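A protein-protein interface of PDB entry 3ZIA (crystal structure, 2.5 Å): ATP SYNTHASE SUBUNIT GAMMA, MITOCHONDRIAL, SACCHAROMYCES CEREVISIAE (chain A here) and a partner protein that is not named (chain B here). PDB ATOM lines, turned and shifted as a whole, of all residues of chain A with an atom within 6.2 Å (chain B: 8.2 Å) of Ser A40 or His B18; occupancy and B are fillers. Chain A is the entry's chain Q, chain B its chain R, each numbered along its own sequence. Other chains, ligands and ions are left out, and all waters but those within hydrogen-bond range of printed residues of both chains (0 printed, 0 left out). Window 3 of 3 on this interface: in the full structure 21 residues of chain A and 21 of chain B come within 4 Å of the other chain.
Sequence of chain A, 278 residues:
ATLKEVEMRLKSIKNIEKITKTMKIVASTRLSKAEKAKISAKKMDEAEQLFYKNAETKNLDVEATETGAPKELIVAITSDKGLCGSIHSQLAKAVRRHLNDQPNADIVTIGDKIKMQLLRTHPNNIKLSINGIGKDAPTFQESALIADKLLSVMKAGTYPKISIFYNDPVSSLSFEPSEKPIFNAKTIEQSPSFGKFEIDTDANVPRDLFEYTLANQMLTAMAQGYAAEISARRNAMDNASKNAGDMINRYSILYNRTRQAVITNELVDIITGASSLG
The backbone carbonyl oxygen (O) of His B18 lies within hydrogen-bond range of the side-chain hydroxyl (OG) of Ser A40 (3.3 Å).
N of Pro B17 lies close to SD of Met A44, 3.4 Å away.
The side-chain hydroxyl (OG) of Ser A40 is in hydrogen-bond range of the backbone carbonyl oxygen (O) of Lys A36.
The backbone carbonyl oxygen (O) of Ala B15 sits at hydrogen-bond distance from the backbone NH (N) of Ala B87 (3.3 Å).
A ring nitrogen (NE2) of His B18 lies within hydrogen-bond range of the side-chain carboxylate (OE1) of Glu B89, 3.2 Å away.
Among the printed residues, merely in contact across the chains: Ser A40 with Pro B17 (3.3 Å), Lys A43 with Thr B20 (3.5 Å), Met A44 with Leu B16 (3.6 Å), Ser A40 with Glu B19 (3.7 Å), Ser A40 with Leu B16 (3.8 Å), Ala A41 with Pro B17 (3.9 Å), Met A44 with Ala B15 (3.9 Å) and Ser A40 with Thr B20 (3.996 Å).
Lys A38 touches none of the printed residues of chain B.
Of the printed residues of chain B, Ser A40 touches Leu B16 (3.8 Å), Pro B17 (3.3 Å), His B18 (3.3 Å), Glu B19 (3.7 Å) and Thr B20 (3.996 Å).
Ala A41 touches just one residue of chain B: Pro B17.
Of the printed residues of chain A, Pro B17 touches Ser A40, Ala A41 and Met A44.
Of chain A, only Ser A40 (3.3 Å) comes within 4 Å of His B18.
Of the printed residues of chain A, Glu B19 touches Ser A40.
Ile B88 touches none of the printed residues of chain A.
The nearest printed residue of chain B that does not touch Ser A40 is Ala B15 (5.3 Å).
The nearest printed residue of chain A that does not touch Thr B20 is Ile A39 (5.2 Å).
Hydrophobic or aromatic side chains of chain B that line the printed part of chain A: Pro B17.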
ATOM      1  N   GLU A  35      16.056  25.511 -14.809  1.00  0.00           N
ATOM      2  CA  GLU A  35      16.961  24.641 -15.565  1.00  0.00           C
ATOM      3  C   GLU A  35      16.311  23.299 -15.853  1.00  0.00           C
ATOM      4  O   GLU A  35      16.360  22.812 -16.982  1.00  0.00           O
ATOM      5  CB  GLU A  35      18.298  24.435 -14.839  1.00  0.00           C
ATOM      6  CG  GLU A  35      19.436  25.326 -15.351  1.00  0.00           C
ATOM      7  CD  GLU A  35      19.902  24.960 -16.761  1.00  0.00           C
ATOM      8  OE1 GLU A  35      20.010  23.749 -17.061  1.00  0.00           O
ATOM      9  OE2 GLU A  35      20.165  25.883 -17.566  1.00  0.00           O
ATOM     10  N   LYS A  36      15.696  22.711 -14.830  1.00  0.00           N
ATOM     11  CA  LYS A  36      15.029  21.421 -14.972  1.00  0.00           C
ATOM     12  C   LYS A  36      13.834  21.461 -15.930  1.00  0.00           C
ATOM     13  O   LYS A  36      13.616  20.518 -16.688  1.00  0.00           O
ATOM     14  CB  LYS A  36      14.637  20.866 -13.603  1.00  0.00           C
ATOM     15  CG  LYS A  36      15.804  20.210 -12.896  1.00  0.00           C
ATOM     16  CD  LYS A  36      15.549  20.014 -11.419  1.00  0.00           C
ATOM     17  CE  LYS A  36      16.614  19.105 -10.821  1.00  0.00           C
ATOM     18  NZ  LYS A  36      16.544  19.052  -9.339  1.00  0.00           N
ATOM     19  N   ALA A  37      13.083  22.561 -15.902  1.00  0.00           N
ATOM     20  CA  ALA A  37      11.947  22.761 -16.807  1.00  0.00           C
ATOM     21  C   ALA A  37      12.390  23.019 -18.248  1.00  0.00           C
ATOM     22  O   ALA A  37      11.626  22.791 -19.183  1.00  0.00           O
ATOM     23  CB  ALA A  37      11.055  23.895 -16.306  1.00  0.00           C
ATOM     24  N   LYS A  38      13.620  23.499 -18.414  1.00  0.00           N
ATOM     25  CA  LYS A  38      14.208  23.729 -19.735  1.00  0.00           C
ATOM     26  C   LYS A  38      14.638  22.408 -20.374  1.00  0.00           C
ATOM     27  O   LYS A  38      14.499  22.225 -21.584  1.00  0.00           O
ATOM     28  CB  LYS A  38      15.400  24.684 -19.630  1.00  0.00           C
ATOM     29  CG  LYS A  38      16.023  25.088 -20.963  1.00  0.00           C
ATOM     30  CD  LYS A  38      17.455  25.598 -20.786  1.00  0.00           C
ATOM     31  CE  LYS A  38      18.468  24.455 -20.689  1.00  0.00           C
ATOM     32  NZ  LYS A  38      19.867  24.948 -20.565  1.00  0.00           N
ATOM     33  N   ILE A  39      15.166  21.501 -19.552  1.00  0.00           N
ATOM     34  CA  ILE A  39      15.542  20.155 -19.991  1.00  0.00           C
ATOM     35  C   ILE A  39      14.301  19.390 -20.463  1.00  0.00           C
ATOM     36  O   ILE A  39      14.307  18.800 -21.546  1.00  0.00           O
ATOM     37  CB  ILE A  39      16.291  19.361 -18.866  1.00  0.00           C
ATOM     38  CG1 ILE A  39      17.613  20.048 -18.469  1.00  0.00           C
ATOM     39  CG2 ILE A  39      16.513  17.891 -19.259  1.00  0.00           C
ATOM     40  CD1 ILE A  39      18.716  20.046 -19.532  1.00  0.00           C
ATOM     41  N   SER A  40      13.242  19.428 -19.652  1.00  0.00           N
ATOM     42  CA  SER A  40      11.961  18.779 -19.961  1.00  0.00           C
ATOM     43  C   SER A  40      11.336  19.280 -21.262  1.00  0.00           C
ATOM     44  O   SER A  40      10.743  18.499 -22.009  1.00  0.00           O
ATOM     45  CB  SER A  40      10.971  18.972 -18.808  1.00  0.00           C
ATOM     46  OG  SER A  40      11.359  18.238 -17.662  1.00  0.00           O
ATOM     47  N   ALA A  41      11.467  20.579 -21.520  1.00  0.00           N
ATOM     48  CA  ALA A  41      10.955  21.185 -22.745  1.00  0.00           C
ATOM     49  C   ALA A  41      11.884  20.930 -23.930  1.00  0.00           C
ATOM     50  O   ALA A  41      11.490  21.118 -25.081  1.00  0.00           O
ATOM     51  CB  ALA A  41      10.736  22.672 -22.551  1.00  0.00           C
ATOM     52  N   LYS A  42      13.112  20.505 -23.645  1.00  0.00           N
ATOM     53  CA  LYS A  42      14.071  20.160 -24.692  1.00  0.00           C
ATOM     54  C   LYS A  42      13.968  18.681 -25.088  1.00  0.00           C
ATOM     55  O   LYS A  42      14.466  18.286 -26.146  1.00  0.00           O
ATOM     56  CB  LYS A  42      15.500  20.514 -24.259  1.00  0.00           C
ATOM     57  CG  LYS A  42      16.428  20.909 -25.408  1.00  0.00           C
ATOM     58  CD  LYS A  42      17.664  21.644 -24.896  1.00  0.00           C
ATOM     59  CE  LYS A  42      18.451  22.276 -26.036  1.00  0.00           C
ATOM     60  NZ  LYS A  42      19.586  23.095 -25.536  1.00  0.00           N
ATOM     61  N   LYS A  43      13.328  17.876 -24.237  1.00  0.00           N
ATOM     62  CA  LYS A  43      13.034  16.470 -24.541  1.00  0.00           C
ATOM     63  C   LYS A  43      11.735  16.364 -25.340  1.00  0.00           C
ATOM     64  O   LYS A  43      11.572  15.460 -26.162  1.00  0.00           O
ATOM     65  CB  LYS A  43      12.925  15.641 -23.262  1.00  0.00           C
ATOM     66  CG  LYS A  43      14.204  15.546 -22.440  1.00  0.00           C
ATOM     67  CD  LYS A  43      14.955  14.246 -22.686  1.00  0.00           C
ATOM     68  CE  LYS A  43      16.116  14.109 -21.707  1.00  0.00           C
ATOM     69  NZ  LYS A  43      16.598  12.710 -21.591  1.00  0.00           N
ATOM     70  N   MET A  44      10.816  17.292 -25.082  1.00  0.00           N
ATOM     71  CA  MET A  44       9.592  17.439 -25.866  1.00  0.00           C
ATOM     72  C   MET A  44       9.872  18.337 -27.079  1.00  0.00           C
ATOM     73  O   MET A  44       9.007  19.082 -27.545  1.00  0.00           O
ATOM     74  CB  MET A  44       8.472  18.009 -24.988  1.00  0.00           C
ATOM     75  CG  MET A  44       7.073  17.863 -25.567  1.00  0.00           C
ATOM     76  SD  MET A  44       5.805  17.832 -24.291  1.00  0.00           S
ATOM     77  CE  MET A  44       4.313  17.936 -25.278  1.00  0.00           C
ATOM     78  N   ASP A  45      11.103  18.253 -27.573  1.00  0.00           N
ATOM     79  CA  ASP A  45      11.555  18.990 -28.746  1.00  0.00           C
ATOM     80  C   ASP A  45      12.377  18.042 -29.616  1.00  0.00           C
ATOM     81  O   ASP A  45      12.430  18.188 -30.840  1.00  0.00           O
ATOM     82  CB  ASP A  45      12.395  20.198 -28.320  1.00  0.00           C
ATOM     83  CG  ASP A  45      12.511  21.253 -29.410  1.00  0.00           C
ATOM     84  OD1 ASP A  45      11.569  21.399 -30.218  1.00  0.00           O
ATOM     85  OD2 ASP A  45      13.546  21.952 -29.447  1.00  0.00           O
ATOM     86  N   ALA B  15       7.214  11.816 -22.816  1.00  0.00           N
ATOM     87  CA  ALA B  15       7.547  13.147 -22.307  1.00  0.00           C
ATOM     88  C   ALA B  15       6.360  14.101 -22.165  1.00  0.00           C
ATOM     89  O   ALA B  15       5.495  14.186 -23.038  1.00  0.00           O
ATOM     90  CB  ALA B  15       8.632  13.785 -23.172  1.00  0.00           C
ATOM     91  N   LEU B  16       6.345  14.819 -21.046  1.00  0.00           N
ATOM     92  CA  LEU B  16       5.410  15.913 -20.805  1.00  0.00           C
ATOM     93  C   LEU B  16       6.219  17.211 -20.789  1.00  0.00           C
ATOM     94  O   LEU B  16       7.445  17.162 -20.659  1.00  0.00           O
ATOM     95  CB  LEU B  16       4.698  15.720 -19.461  1.00  0.00           C
ATOM     96  CG  LEU B  16       3.706  14.577 -19.221  1.00  0.00           C
ATOM     97  CD1 LEU B  16       4.388  13.219 -19.166  1.00  0.00           C
ATOM     98  CD2 LEU B  16       2.970  14.827 -17.923  1.00  0.00           C
ATOM     99  N   PRO B  17       5.548  18.376 -20.923  1.00  0.00           N
ATOM    100  CA  PRO B  17       6.269  19.651 -20.845  1.00  0.00           C
ATOM    101  C   PRO B  17       7.070  19.849 -19.552  1.00  0.00           C
ATOM    102  O   PRO B  17       8.138  20.460 -19.582  1.00  0.00           O
ATOM    103  CB  PRO B  17       5.151  20.701 -20.944  1.00  0.00           C
ATOM    104  CG  PRO B  17       3.867  19.956 -20.808  1.00  0.00           C
ATOM    105  CD  PRO B  17       4.139  18.582 -21.296  1.00  0.00           C
ATOM    106  N   HIS B  18       6.565  19.325 -18.438  1.00  0.00           N
ATOM    107  CA  HIS B  18       7.162  19.558 -17.122  1.00  0.00           C
ATOM    108  C   HIS B  18       7.981  18.384 -16.584  1.00  0.00           C
ATOM    109  O   HIS B  18       8.759  18.549 -15.645  1.00  0.00           O
ATOM    110  CB  HIS B  18       6.076  19.944 -16.112  1.00  0.00           C
ATOM    111  CG  HIS B  18       4.962  18.946 -16.007  1.00  0.00           C
ATOM    112  ND1 HIS B  18       5.016  17.853 -15.170  1.00  0.00           N
ATOM    113  CD2 HIS B  18       3.761  18.882 -16.631  1.00  0.00           C
ATOM    114  CE1 HIS B  18       3.899  17.157 -15.282  1.00  0.00           C
ATOM    115  NE2 HIS B  18       3.121  17.760 -16.162  1.00  0.00           N
ATOM    116  N   GLU B  19       7.801  17.206 -17.180  1.00  0.00           N
ATOM    117  CA  GLU B  19       8.448  15.982 -16.703  1.00  0.00           C
ATOM    118  C   GLU B  19       8.566  14.956 -17.825  1.00  0.00           C
ATOM    119  O   GLU B  19       7.655  14.807 -18.638  1.00  0.00           O
ATOM    120  CB  GLU B  19       7.658  15.392 -15.529  1.00  0.00           C
ATOM    121  CG  GLU B  19       8.345  14.247 -14.800  1.00  0.00           C
ATOM    122  CD  GLU B  19       7.544  13.733 -13.616  1.00  0.00           C
ATOM    123  OE1 GLU B  19       6.541  14.377 -13.237  1.00  0.00           O
ATOM    124  OE2 GLU B  19       7.924  12.683 -13.056  1.00  0.00           O
ATOM    125  N   THR B  20       9.692  14.246 -17.865  1.00  0.00           N
ATOM    126  CA  THR B  20       9.908  13.207 -18.870  1.00  0.00           C
ATOM    127  C   THR B  20       9.979  11.831 -18.203  1.00  0.00           C
ATOM    128  O   THR B  20      10.976  11.482 -17.563  1.00  0.00           O
ATOM    129  CB  THR B  20      11.161  13.487 -19.727  1.00  0.00           C
ATOM    130  OG1 THR B  20      12.329  13.466 -18.899  1.00  0.00           O
ATOM    131  CG2 THR B  20      11.046  14.851 -20.407  1.00  0.00           C
ATOM    132  N   LEU B  21       8.907  11.059 -18.370  1.00  0.00           N
ATOM    133  CA  LEU B  21       8.691   9.821 -17.615  1.00  0.00           C
ATOM    134  C   LEU B  21       9.560   8.624 -18.008  1.00  0.00           C
ATOM    135  O   LEU B  21       9.891   7.801 -17.152  1.00  0.00           O
ATOM    136  CB  LEU B  21       7.208   9.423 -17.646  1.00  0.00           C
ATOM    137  CG  LEU B  21       6.219  10.222 -16.782  1.00  0.00           C
ATOM    138  CD1 LEU B  21       4.791   9.990 -17.254  1.00  0.00           C
ATOM    139  CD2 LEU B  21       6.351   9.902 -15.283  1.00  0.00           C
ATOM    140  N   ALA B  87       2.342  14.173 -24.169  1.00  0.00           N
ATOM    141  CA  ALA B  87       1.093  14.630 -23.561  1.00  0.00           C
ATOM    142  C   ALA B  87       1.353  15.766 -22.582  1.00  0.00           C
ATOM    143  O   ALA B  87       2.408  15.817 -21.954  1.00  0.00           O
ATOM    144  CB  ALA B  87       0.386  13.479 -22.861  1.00  0.00           C
ATOM    145  N   ILE B  88       0.379  16.664 -22.460  1.00  0.00           N
ATOM    146  CA  ILE B  88       0.458  17.806 -21.548  1.00  0.00           C
ATOM    147  C   ILE B  88       0.406  17.366 -20.083  1.00  0.00           C
ATOM    148  O   ILE B  88       1.288  17.713 -19.299  1.00  0.00           O
ATOM    149  CB  ILE B  88      -0.639  18.834 -21.861  1.00  0.00           C
ATOM    150  CG1 ILE B  88      -0.440  19.371 -23.273  1.00  0.00           C
ATOM    151  CG2 ILE B  88      -0.619  19.979 -20.865  1.00  0.00           C
ATOM    152  CD1 ILE B  88      -1.681  19.323 -24.097  1.00  0.00           C
ATOM    153  N   GLU B  89      -0.623  16.608 -19.719  1.00  0.00           N
ATOM    154  CA  GLU B  89      -0.698  16.008 -18.388  1.00  0.00           C
ATOM    155  C   GLU B  89      -0.772  14.490 -18.471  1.00  0.00           C
ATOM    156  O   GLU B  89      -1.330  13.939 -19.421  1.00  0.00           O
ATOM    157  CB  GLU B  89      -1.900  16.541 -17.602  1.00  0.00           C
ATOM    158  CG  GLU B  89      -1.838  18.021 -17.253  1.00  0.00           C
ATOM    159  CD  GLU B  89      -0.706  18.391 -16.300  1.00  0.00           C
ATOM    160  OE1 GLU B  89      -0.075  17.495 -15.692  1.00  0.00           O
ATOM    161  OE2 GLU B  89      -0.453  19.601 -16.163  1.00  0.00           O
ATOM    162  N   ALA B  90      -0.202  13.828 -17.469  1.00  0.00           N
ATOM    163  CA  ALA B  90      -0.228  12.376 -17.365  1.00  0.00           C
ATOM    164  C   ALA B  90      -0.017  11.987 -15.914  1.00  0.00           C
ATOM    165  O   ALA B  90       0.973  12.386 -15.299  1.00  0.00           O
ATOM    166  CB  ALA B  90       0.842  11.756 -18.244  1.00  0.00           C
ATOM    167  N   PHE B  91      -0.956  11.219 -15.368  1.00  0.00           N
ATOM    168  CA  PHE B  91      -0.925  10.819 -13.960  1.00  0.00           C
ATOM    169  C   PHE B  91      -1.448   9.402 -13.738  1.00  0.00           C
ATOM    170  O   PHE B  91      -2.329   8.945 -14.472  1.00  0.00           O
ATOM    171  CB  PHE B  91      -1.764  11.780 -13.107  1.00  0.00           C
ATOM    172  CG  PHE B  91      -1.168  13.149 -12.962  1.00  0.00           C
ATOM    173  CD1 PHE B  91      -0.045  13.354 -12.161  1.00  0.00           C
ATOM    174  CD2 PHE B  91      -1.734  14.238 -13.618  1.00  0.00           C
ATOM    175  CE1 PHE B  91       0.511  14.622 -12.024  1.00  0.00           C
ATOM    176  CE2 PHE B  91      -1.189  15.513 -13.486  1.00  0.00           C
ATOM    177  CZ  PHE B  91      -0.064  15.705 -12.688  1.00  0.00           C
